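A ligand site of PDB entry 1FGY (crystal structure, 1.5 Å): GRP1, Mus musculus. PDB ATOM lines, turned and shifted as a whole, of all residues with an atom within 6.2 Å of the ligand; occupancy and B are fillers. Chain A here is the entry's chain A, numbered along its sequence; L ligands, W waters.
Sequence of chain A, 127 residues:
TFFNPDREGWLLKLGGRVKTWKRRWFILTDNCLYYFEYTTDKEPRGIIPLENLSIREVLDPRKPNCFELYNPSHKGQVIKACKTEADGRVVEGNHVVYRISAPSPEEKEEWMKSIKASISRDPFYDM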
ATOM      1  N   LYS A  13      22.807 -20.689 -23.258  1.00  0.00           N
ATOM      2  CA  LYS A  13      22.625 -19.246 -23.267  1.00  0.00           C
ATOM      3  C   LYS A  13      23.470 -18.576 -24.334  1.00  0.00           C
ATOM      4  O   LYS A  13      24.613 -18.973 -24.571  1.00  0.00           O
ATOM      5  CB  LYS A  13      22.942 -18.638 -21.888  1.00  0.00           C
ATOM      6  CG  LYS A  13      24.309 -19.018 -21.319  1.00  0.00           C
ATOM      7  CD  LYS A  13      24.615 -18.237 -20.038  1.00  0.00           C
ATOM      8  CE  LYS A  13      24.914 -16.770 -20.321  1.00  0.00           C
ATOM      9  NZ  LYS A  13      26.162 -16.626 -21.106  1.00  0.00           N
ATOM     10  N   LEU A  14      22.872 -17.604 -25.012  1.00  0.00           N
ATOM     11  CA  LEU A  14      23.567 -16.853 -26.057  1.00  0.00           C
ATOM     12  C   LEU A  14      24.334 -15.709 -25.384  1.00  0.00           C
ATOM     13  O   LEU A  14      23.800 -15.037 -24.487  1.00  0.00           O
ATOM     14  CB  LEU A  14      22.567 -16.312 -27.079  1.00  0.00           C
ATOM     15  CG  LEU A  14      23.128 -15.551 -28.281  1.00  0.00           C
ATOM     16  CD1 LEU A  14      24.004 -16.471 -29.120  1.00  0.00           C
ATOM     17  CD2 LEU A  14      21.974 -14.994 -29.108  1.00  0.00           C
ATOM     18  N   GLY A  15      25.584 -15.503 -25.799  1.00  0.00           N
ATOM     19  CA  GLY A  15      26.412 -14.447 -25.226  1.00  0.00           C
ATOM     20  C   GLY A  15      25.917 -13.019 -25.425  1.00  0.00           C
ATOM     21  O   GLY A  15      24.965 -12.774 -26.179  1.00  0.00           O
ATOM     22  N   GLY A  16      26.582 -12.074 -24.763  1.00  0.00           N
ATOM     23  CA  GLY A  16      26.200 -10.673 -24.848  1.00  0.00           C
ATOM     24  C   GLY A  16      26.732  -9.983 -26.082  1.00  0.00           C
ATOM     25  O   GLY A  16      26.093 -10.015 -27.138  1.00  0.00           O
ATOM     26  N   ARG A  17      27.866  -9.304 -25.943  1.00  0.00           N
ATOM     27  CA  ARG A  17      28.498  -8.615 -27.073  1.00  0.00           C
ATOM     28  C   ARG A  17      28.862  -9.699 -28.089  1.00  0.00           C
ATOM     29  O   ARG A  17      28.528  -9.594 -29.262  1.00  0.00           O
ATOM     30  CB  ARG A  17      29.750  -7.869 -26.621  1.00  0.00           C
ATOM     31  CG  ARG A  17      29.471  -6.668 -25.749  1.00  0.00           C
ATOM     32  CD  ARG A  17      30.758  -5.929 -25.417  1.00  0.00           C
ATOM     33  NE  ARG A  17      30.499  -4.714 -24.651  1.00  0.00           N
ATOM     34  CZ  ARG A  17      31.203  -4.328 -23.587  1.00  0.00           C
ATOM     35  NH1 ARG A  17      32.211  -5.077 -23.146  1.00  0.00           N
ATOM     36  NH2 ARG A  17      30.876  -3.218 -22.940  1.00  0.00           N
ATOM     37  N   VAL A  18      29.566 -10.731 -27.612  1.00  0.00           N
ATOM     38  CA  VAL A  18      29.952 -11.837 -28.474  1.00  0.00           C
ATOM     39  C   VAL A  18      28.799 -12.827 -28.447  1.00  0.00           C
ATOM     40  O   VAL A  18      28.449 -13.366 -27.387  1.00  0.00           O
ATOM     41  CB  VAL A  18      31.244 -12.506 -27.991  1.00  0.00           C
ATOM     42  CG1 VAL A  18      31.600 -13.692 -28.890  1.00  0.00           C
ATOM     43  CG2 VAL A  18      32.391 -11.492 -27.986  1.00  0.00           C
ATOM     44  N   LYS A  19      28.195 -13.048 -29.601  1.00  0.00           N
ATOM     45  CA  LYS A  19      27.042 -13.944 -29.736  1.00  0.00           C
ATOM     46  C   LYS A  19      27.373 -15.424 -29.882  1.00  0.00           C
ATOM     47  O   LYS A  19      27.155 -16.017 -30.935  1.00  0.00           O
ATOM     48  CB  LYS A  19      26.178 -13.490 -30.912  1.00  0.00           C
ATOM     49  CG  LYS A  19      25.752 -12.024 -30.855  1.00  0.00           C
ATOM     50  CD  LYS A  19      24.904 -11.730 -29.631  1.00  0.00           C
ATOM     51  CE  LYS A  19      24.341 -10.319 -29.682  1.00  0.00           C
ATOM     52  NZ  LYS A  19      25.408  -9.273 -29.587  1.00  0.00           N
ATOM     53  N   THR A  20      27.861 -16.023 -28.798  1.00  0.00           N
ATOM     54  CA  THR A  20      28.187 -17.448 -28.788  1.00  0.00           C
ATOM     55  C   THR A  20      27.319 -18.185 -27.767  1.00  0.00           C
ATOM     56  O   THR A  20      26.996 -17.649 -26.720  1.00  0.00           O
ATOM     57  CB  THR A  20      29.684 -17.703 -28.460  1.00  0.00           C
ATOM     58  OG1 THR A  20      30.041 -17.037 -27.249  1.00  0.00           O
ATOM     59  CG2 THR A  20      30.573 -17.219 -29.606  1.00  0.00           C
ATOM     60  N   TRP A  21      26.901 -19.393 -28.132  1.00  0.00           N
ATOM     61  CA  TRP A  21      26.064 -20.214 -27.253  1.00  0.00           C
ATOM     62  C   TRP A  21      26.940 -21.018 -26.309  1.00  0.00           C
ATOM     63  O   TRP A  21      27.894 -21.661 -26.728  1.00  0.00           O
ATOM     64  CB  TRP A  21      25.219 -21.182 -28.073  1.00  0.00           C
ATOM     65  CG  TRP A  21      24.093 -20.528 -28.847  1.00  0.00           C
ATOM     66  CD1 TRP A  21      24.113 -20.171 -30.167  1.00  0.00           C
ATOM     67  CD2 TRP A  21      22.786 -20.212 -28.352  1.00  0.00           C
ATOM     68  NE1 TRP A  21      22.899 -19.651 -30.528  1.00  0.00           N
ATOM     69  CE2 TRP A  21      22.063 -19.658 -29.441  1.00  0.00           C
ATOM     70  CE3 TRP A  21      22.155 -20.336 -27.106  1.00  0.00           C
ATOM     71  CZ2 TRP A  21      20.732 -19.235 -29.309  1.00  0.00           C
ATOM     72  CZ3 TRP A  21      20.839 -19.911 -26.991  1.00  0.00           C
ATOM     73  CH2 TRP A  21      20.137 -19.369 -28.082  1.00  0.00           C
ATOM     74  N   LYS A  22      26.589 -20.989 -25.019  1.00  0.00           N
ATOM     75  CA  LYS A  22      27.331 -21.709 -23.991  1.00  0.00           C
ATOM     76  C   LYS A  22      26.377 -22.527 -23.130  1.00  0.00           C
ATOM     77  O   LYS A  22      25.270 -22.083 -22.814  1.00  0.00           O
ATOM     78  CB  LYS A  22      28.101 -20.737 -23.093  1.00  0.00           C
ATOM     79  CG  LYS A  22      29.149 -19.892 -23.792  1.00  0.00           C
ATOM     80  CD  LYS A  22      30.268 -20.762 -24.332  1.00  0.00           C
ATOM     81  CE  LYS A  22      31.309 -19.937 -25.068  1.00  0.00           C
ATOM     82  NZ  LYS A  22      32.380 -20.818 -25.615  1.00  0.00           N
ATOM     83  N   ARG A  24      25.336 -23.942 -19.730  1.00  0.00           N
ATOM     84  CA  ARG A  24      25.540 -23.571 -18.335  1.00  0.00           C
ATOM     85  C   ARG A  24      24.512 -24.226 -17.413  1.00  0.00           C
ATOM     86  O   ARG A  24      23.394 -24.531 -17.834  1.00  0.00           O
ATOM     87  CB  ARG A  24      25.439 -22.044 -18.192  1.00  0.00           C
ATOM     88  CG  ARG A  24      26.446 -21.230 -19.031  1.00  0.00           C
ATOM     89  CD  ARG A  24      27.873 -21.400 -18.499  1.00  0.00           C
ATOM     90  NE  ARG A  24      28.875 -20.681 -19.288  1.00  0.00           N
ATOM     91  CZ  ARG A  24      29.805 -21.267 -20.041  1.00  0.00           C
ATOM     92  NH1 ARG A  24      29.880 -22.587 -20.117  1.00  0.00           N
ATOM     93  NH2 ARG A  24      30.702 -20.519 -20.674  1.00  0.00           N
ATOM     94  N   TYR A  35      24.208 -18.828 -12.965  1.00  0.00           N
ATOM     95  CA  TYR A  35      24.664 -19.832 -13.904  1.00  0.00           C
ATOM     96  C   TYR A  35      26.132 -20.166 -13.657  1.00  0.00           C
ATOM     97  O   TYR A  35      26.906 -19.320 -13.210  1.00  0.00           O
ATOM     98  CB  TYR A  35      24.372 -19.462 -15.360  1.00  0.00           C
ATOM     99  CG  TYR A  35      24.875 -18.121 -15.815  1.00  0.00           C
ATOM    100  CD1 TYR A  35      26.055 -18.019 -16.551  1.00  0.00           C
ATOM    101  CD2 TYR A  35      24.152 -16.963 -15.552  1.00  0.00           C
ATOM    102  CE1 TYR A  35      26.499 -16.778 -17.026  1.00  0.00           C
ATOM    103  CE2 TYR A  35      24.579 -15.721 -16.018  1.00  0.00           C
ATOM    104  CZ  TYR A  35      25.768 -15.641 -16.755  1.00  0.00           C
ATOM    105  OH  TYR A  35      26.195 -14.421 -17.217  1.00  0.00           O
ATOM    106  N   ARG A  45      29.296 -18.379 -12.653  1.00  0.00           N
ATOM    107  CA  ARG A  45      29.908 -17.677 -13.781  1.00  0.00           C
ATOM    108  C   ARG A  45      29.213 -16.305 -13.880  1.00  0.00           C
ATOM    109  O   ARG A  45      29.847 -15.307 -14.219  1.00  0.00           O
ATOM    110  CB  ARG A  45      29.682 -18.477 -15.080  1.00  0.00           C
ATOM    111  CG  ARG A  45      30.088 -17.769 -16.380  1.00  0.00           C
ATOM    112  CD  ARG A  45      31.549 -17.326 -16.387  1.00  0.00           C
ATOM    113  NE  ARG A  45      32.480 -18.428 -16.108  1.00  0.00           N
ATOM    114  CZ  ARG A  45      32.995 -19.246 -17.033  1.00  0.00           C
ATOM    115  NH1 ARG A  45      32.680 -19.105 -18.316  1.00  0.00           N
ATOM    116  NH2 ARG A  45      33.846 -20.187 -16.679  1.00  0.00           N
ATOM    117  N   GLY A  46      27.929 -16.271 -13.520  1.00  0.00           N
ATOM    118  CA  GLY A  46      27.168 -15.030 -13.554  1.00  0.00           C
ATOM    119  C   GLY A  46      25.875 -15.044 -12.764  1.00  0.00           C
ATOM    120  O   GLY A  46      25.426 -16.091 -12.270  1.00  0.00           O
ATOM    121  N   LYS A  83      28.920 -10.854 -14.077  1.00  0.00           N
ATOM    122  CA  LYS A  83      29.569 -12.115 -14.421  1.00  0.00           C
ATOM    123  C   LYS A  83      31.069 -12.017 -14.251  1.00  0.00           C
ATOM    124  O   LYS A  83      31.624 -10.927 -14.085  1.00  0.00           O
ATOM    125  CB  LYS A  83      29.205 -12.534 -15.854  1.00  0.00           C
ATOM    126  CG  LYS A  83      30.115 -11.992 -16.957  1.00  0.00           C
ATOM    127  CD  LYS A  83      29.784 -10.576 -17.376  1.00  0.00           C
ATOM    128  CE  LYS A  83      30.579 -10.185 -18.626  1.00  0.00           C
ATOM    129  NZ  LYS A  83      30.352 -11.133 -19.757  1.00  0.00           N
ATOM    130  N   THR A  84      31.733 -13.171 -14.250  1.00  0.00           N
ATOM    131  CA  THR A  84      33.183 -13.214 -14.105  1.00  0.00           C
ATOM    132  C   THR A  84      33.873 -13.398 -15.453  1.00  0.00           C
ATOM    133  O   THR A  84      33.255 -13.818 -16.440  1.00  0.00           O
ATOM    134  CB  THR A  84      33.647 -14.347 -13.163  1.00  0.00           C
ATOM    135  OG1 THR A  84      33.300 -15.617 -13.736  1.00  0.00           O
ATOM    136  CG2 THR A  84      32.994 -14.215 -11.802  1.00  0.00           C
ATOM    137  N   GLU A  85      35.140 -13.008 -15.498  1.00  0.00           N
ATOM    138  CA  GLU A  85      35.968 -13.151 -16.686  1.00  0.00           C
ATOM    139  C   GLU A  85      37.114 -14.057 -16.286  1.00  0.00           C
ATOM    140  O   GLU A  85      37.492 -14.116 -15.117  1.00  0.00           O
ATOM    141  CB  GLU A  85      36.506 -11.785 -17.137  1.00  0.00           C
ATOM    142  CG  GLU A  85      35.453 -10.807 -17.632  1.00  0.00           C
ATOM    143  CD  GLU A  85      34.844 -11.176 -18.980  1.00  0.00           C
ATOM    144  OE1 GLU A  85      35.111 -12.291 -19.489  1.00  0.00           O
ATOM    145  OE2 GLU A  85      34.097 -10.358 -19.531  1.00  0.00           O
ATOM    146  N   GLY A  93      27.075  -7.179 -16.917  1.00  0.00           N
ATOM    147  CA  GLY A  93      26.755  -7.779 -18.201  1.00  0.00           C
ATOM    148  C   GLY A  93      26.474  -6.739 -19.262  1.00  0.00           C
ATOM    149  O   GLY A  93      26.180  -5.582 -18.943  1.00  0.00           O
ATOM    150  N   ASN A  94      26.521  -7.153 -20.528  1.00  0.00           N
ATOM    151  CA  ASN A  94      26.279  -6.274 -21.680  1.00  0.00           C
ATOM    152  C   ASN A  94      25.036  -6.672 -22.476  1.00  0.00           C
ATOM    153  O   ASN A  94      24.841  -6.204 -23.600  1.00  0.00           O
ATOM    154  CB  ASN A  94      27.490  -6.300 -22.630  1.00  0.00           C
ATOM    155  CG  ASN A  94      28.795  -6.035 -21.927  1.00  0.00           C
ATOM    156  OD1 ASN A  94      28.969  -4.997 -21.277  1.00  0.00           O
ATOM    157  ND2 ASN A  94      29.727  -6.974 -22.037  1.00  0.00           N
ATOM    158  N   HIS A  95      24.177  -7.506 -21.898  1.00  0.00           N
ATOM    159  CA  HIS A  95      22.968  -7.969 -22.582  1.00  0.00           C
ATOM    160  C   HIS A  95      21.779  -7.022 -22.587  1.00  0.00           C
ATOM    161  O   HIS A  95      21.486  -6.374 -21.584  1.00  0.00           O
ATOM    162  CB  HIS A  95      22.457  -9.271 -21.952  1.00  0.00           C
ATOM    163  CG  HIS A  95      23.335 -10.474 -22.181  1.00  0.00           C
ATOM    164  ND1 HIS A  95      22.957 -11.519 -22.997  1.00  0.00           N
ATOM    165  CD2 HIS A  95      24.515 -10.832 -21.617  1.00  0.00           C
ATOM    166  CE1 HIS A  95      23.851 -12.480 -22.916  1.00  0.00           C
ATOM    167  NE2 HIS A  95      24.815 -12.088 -22.084  1.00  0.00           N
ATOM    168  N   TYR A  98      18.503 -11.877 -22.969  1.00  0.00           N
ATOM    169  CA  TYR A  98      19.166 -13.135 -22.684  1.00  0.00           C
ATOM    170  C   TYR A  98      18.376 -14.209 -23.415  1.00  0.00           C
ATOM    171  O   TYR A  98      17.229 -14.490 -23.057  1.00  0.00           O
ATOM    172  CB  TYR A  98      19.185 -13.441 -21.183  1.00  0.00           C
ATOM    173  CG  TYR A  98      20.257 -12.725 -20.416  1.00  0.00           C
ATOM    174  CD1 TYR A  98      20.014 -11.485 -19.841  1.00  0.00           C
ATOM    175  CD2 TYR A  98      21.538 -13.278 -20.297  1.00  0.00           C
ATOM    176  CE1 TYR A  98      21.015 -10.800 -19.156  1.00  0.00           C
ATOM    177  CE2 TYR A  98      22.541 -12.605 -19.606  1.00  0.00           C
ATOM    178  CZ  TYR A  98      22.280 -11.368 -19.047  1.00  0.00           C
ATOM    179  OH  TYR A  98      23.263 -10.687 -18.379  1.00  0.00           O
HETATM  180  C1  LIG L   1      31.363 -15.111 -24.278  1.00  0.00           C
HETATM  181  O1  LIG L   1      31.662 -15.696 -25.524  1.00  0.00           O
HETATM  182  C2  LIG L   1      30.464 -16.078 -23.523  1.00  0.00           C
HETATM  183  O2  LIG L   1      29.285 -16.315 -24.293  1.00  0.00           O
HETATM  184  C3  LIG L   1      30.105 -15.501 -22.164  1.00  0.00           C
HETATM  185  O3  LIG L   1      29.243 -16.404 -21.483  1.00  0.00           O
HETATM  186  C4  LIG L   1      29.411 -14.164 -22.331  1.00  0.00           C
HETATM  187  O4  LIG L   1      29.101 -13.655 -21.026  1.00  0.00           O
HETATM  188  C5  LIG L   1      30.291 -13.174 -23.081  1.00  0.00           C
HETATM  189  O5  LIG L   1      29.529 -11.964 -23.239  1.00  0.00           O
HETATM  190  C6  LIG L   1      30.679 -13.742 -24.450  1.00  0.00           C
HETATM  191  O6  LIG L   1      31.707 -12.929 -25.015  1.00  0.00           O
HETATM  192  P1  LIG L   1      33.136 -16.158 -25.922  1.00  0.00           P
HETATM  193  O7  LIG L   1      33.048 -16.747 -27.278  1.00  0.00           O
HETATM  194  O8  LIG L   1      33.479 -17.127 -24.853  1.00  0.00           O
HETATM  195  O9  LIG L   1      33.989 -14.947 -25.887  1.00  0.00           O
HETATM  196  P2  LIG L   1      29.591 -17.007 -20.047  1.00  0.00           P
HETATM  197  O10 LIG L   1      28.444 -17.889 -19.669  1.00  0.00           O
HETATM  198  O11 LIG L   1      30.859 -17.738 -20.287  1.00  0.00           O
HETATM  199  O12 LIG L   1      29.779 -15.870 -19.099  1.00  0.00           O
HETATM  200  P3  LIG L   1      27.614 -13.462 -20.426  1.00  0.00           P
HETATM  201  O13 LIG L   1      26.636 -13.851 -21.466  1.00  0.00           O
HETATM  202  O14 LIG L   1      27.654 -14.375 -19.257  1.00  0.00           O
HETATM  203  O15 LIG L   1      27.505 -12.051 -19.989  1.00  0.00           O
HETATM  204  P4  LIG L   1      30.166 -10.494 -23.425  1.00  0.00           P
HETATM  205  O16 LIG L   1      31.095 -10.265 -22.303  1.00  0.00           O
HETATM  206  O17 LIG L   1      29.040  -9.523 -23.438  1.00  0.00           O
HETATM  207  O18 LIG L   1      30.813 -10.581 -24.757  1.00  0.00           O
HETATM  208  O   HOH W   1      33.900 -11.308 -22.341  1.00  0.00           O
HETATM  209  O   HOH W   2      27.453  -9.652 -21.157  1.00  0.00           O
HETATM  210  O   HOH W   3      34.834 -16.305 -29.315  1.00  0.00           O
HETATM  211  O   HOH W   4      33.015  -8.803 -25.548  1.00  0.00           O
HETATM  212  O   HOH W   5      25.699 -11.620 -17.999  1.00  0.00           O
HETATM  213  O   HOH W   6      32.517  -8.040 -21.408  1.00  0.00           O
HETATM  214  O   HOH W   7      26.839 -17.478 -23.504  1.00  0.00           O
HETATM  215  O   HOH W   8      33.648 -19.288 -27.736  1.00  0.00           O
HETATM  216  O   HOH W   9      31.866 -13.791 -18.916  1.00  0.00           O
HETATM  217  O   HOH W  10      33.444 -16.969 -20.809  1.00  0.00           O
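A ring nitrogen (NE2) of His 95 is in hydrogen-bond range of an oxygen (O13) of the ligand, at 2.6 Å.
N of Gly 16 lies within hydrogen-bond range of O5 of the ligand (3.3 Å).
An oxygen (O11) of the ligand lies within salt-bridge range of the guanidinium group of Arg 45 (3.0 Å).
The side-chain amino group of Lys 83 lies within salt-bridge range of an oxygen (O16) of the ligand (2.8 Å).
An oxygen (O1) of the ligand is in hydrogen-bond range of the side-chain hydroxyl (OG1) of Thr 20 (2.7 Å).
NH2 of Arg 24 lies within salt-bridge range of O11 of the ligand (2.8 Å).
The side-chain amino group of Lys 22 lies within salt-bridge range of an oxygen (O8) of the ligand (3.9 Å).
O18 of the ligand sits at hydrogen-bond distance from N of Val 18 (3.1 Å).
N of Arg 17 sits at hydrogen-bond distance from O17 of the ligand.
The side-chain amide nitrogen of Asn 94 lies within hydrogen-bond range of an oxygen (O17) of the ligand (3.0 Å).
OH of Tyr 35 is in hydrogen-bond range of O14 of the ligand.
NZ of Lys 13 lies within salt-bridge range of O13 of the ligand (2.8 Å).
The side-chain amide oxygen (OD1) of Asn 94 lies within hydrogen-bond range of the guanidinium group (NH2) of Arg 17 (3.1 Å).
O of Gly 46 is in hydrogen-bond range of N of Tyr 35, at 3.1 Å.
NE2 of His 95 sits at hydrogen-bond distance from N of Gly 16 (3.2 Å).
O of Thr 20 lies within hydrogen-bond range of N of Gly 15.
The backbone carbonyl oxygen (O) of Tyr 35 lies within hydrogen-bond range of the backbone NH (N) of Arg 45.
O of Lys 13 is in hydrogen-bond range of N of Lys 22 (2.9 Å).
The backbone carbonyl oxygen (O) of Gly 16 is in hydrogen-bond range of the side-chain amino group (NZ) of Lys 19 (2.6 Å).
The backbone NH of Thr 84 sits at hydrogen-bond distance from the backbone carbonyl oxygen of Arg 45, 2.8 Å away.
Gly 15 touches the ligand (CA to O2, 3.6 Å).
Hydrophobic or aromatic side chains that line the ligand: Val 18, Tyr 35 and His 95.
Within 4 Å of the ligand: Lys 13, Gly 15, Gly 16, Arg 17, Val 18, Thr 20, Lys 22, Arg 24, Tyr 35, Arg 45, Lys 83, Asn 94 and His 95.
The nearest printed residue that does not touch the ligand is Glu 85 (4.1 Å).
Water W2 bridges O15 of the ligand (2.7 Å) and N of Asn 94 (2.7 Å).
Water W5 lies within hydrogen-bond range of the side-chain hydroxyl of Tyr 98 (2.6 Å), an oxygen (O15) of the ligand (2.7 Å) and the side-chain hydroxyl of Tyr 35 (3.0 Å).
Water W10 lies within hydrogen-bond range of an oxygen (O11) of the ligand (2.7 Å) and the guanidinium group (NH1) of Arg 45 (3.4 Å).
Water W6 lies within hydrogen-bond range of an oxygen (O16) of the ligand (2.8 Å), the side-chain amide nitrogen of Asn 94 (3.1 Å), the side-chain carboxylate of Glu 85 (3.4 Å) and the guanidinium group of Arg 17 (3.4 Å).
Water W9 lies within hydrogen-bond range of the backbone carbonyl oxygen (O) of Thr 84 (2.8 Å), an oxygen (O12) of the ligand (3.0 Å) and the side-chain amino group (NZ) of Lys 83 (3.2 Å).
Water W1 bridges the side-chain carboxylate of Glu 85 (3.0 Å) and an oxygen (O16) of the ligand (3.0 Å).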
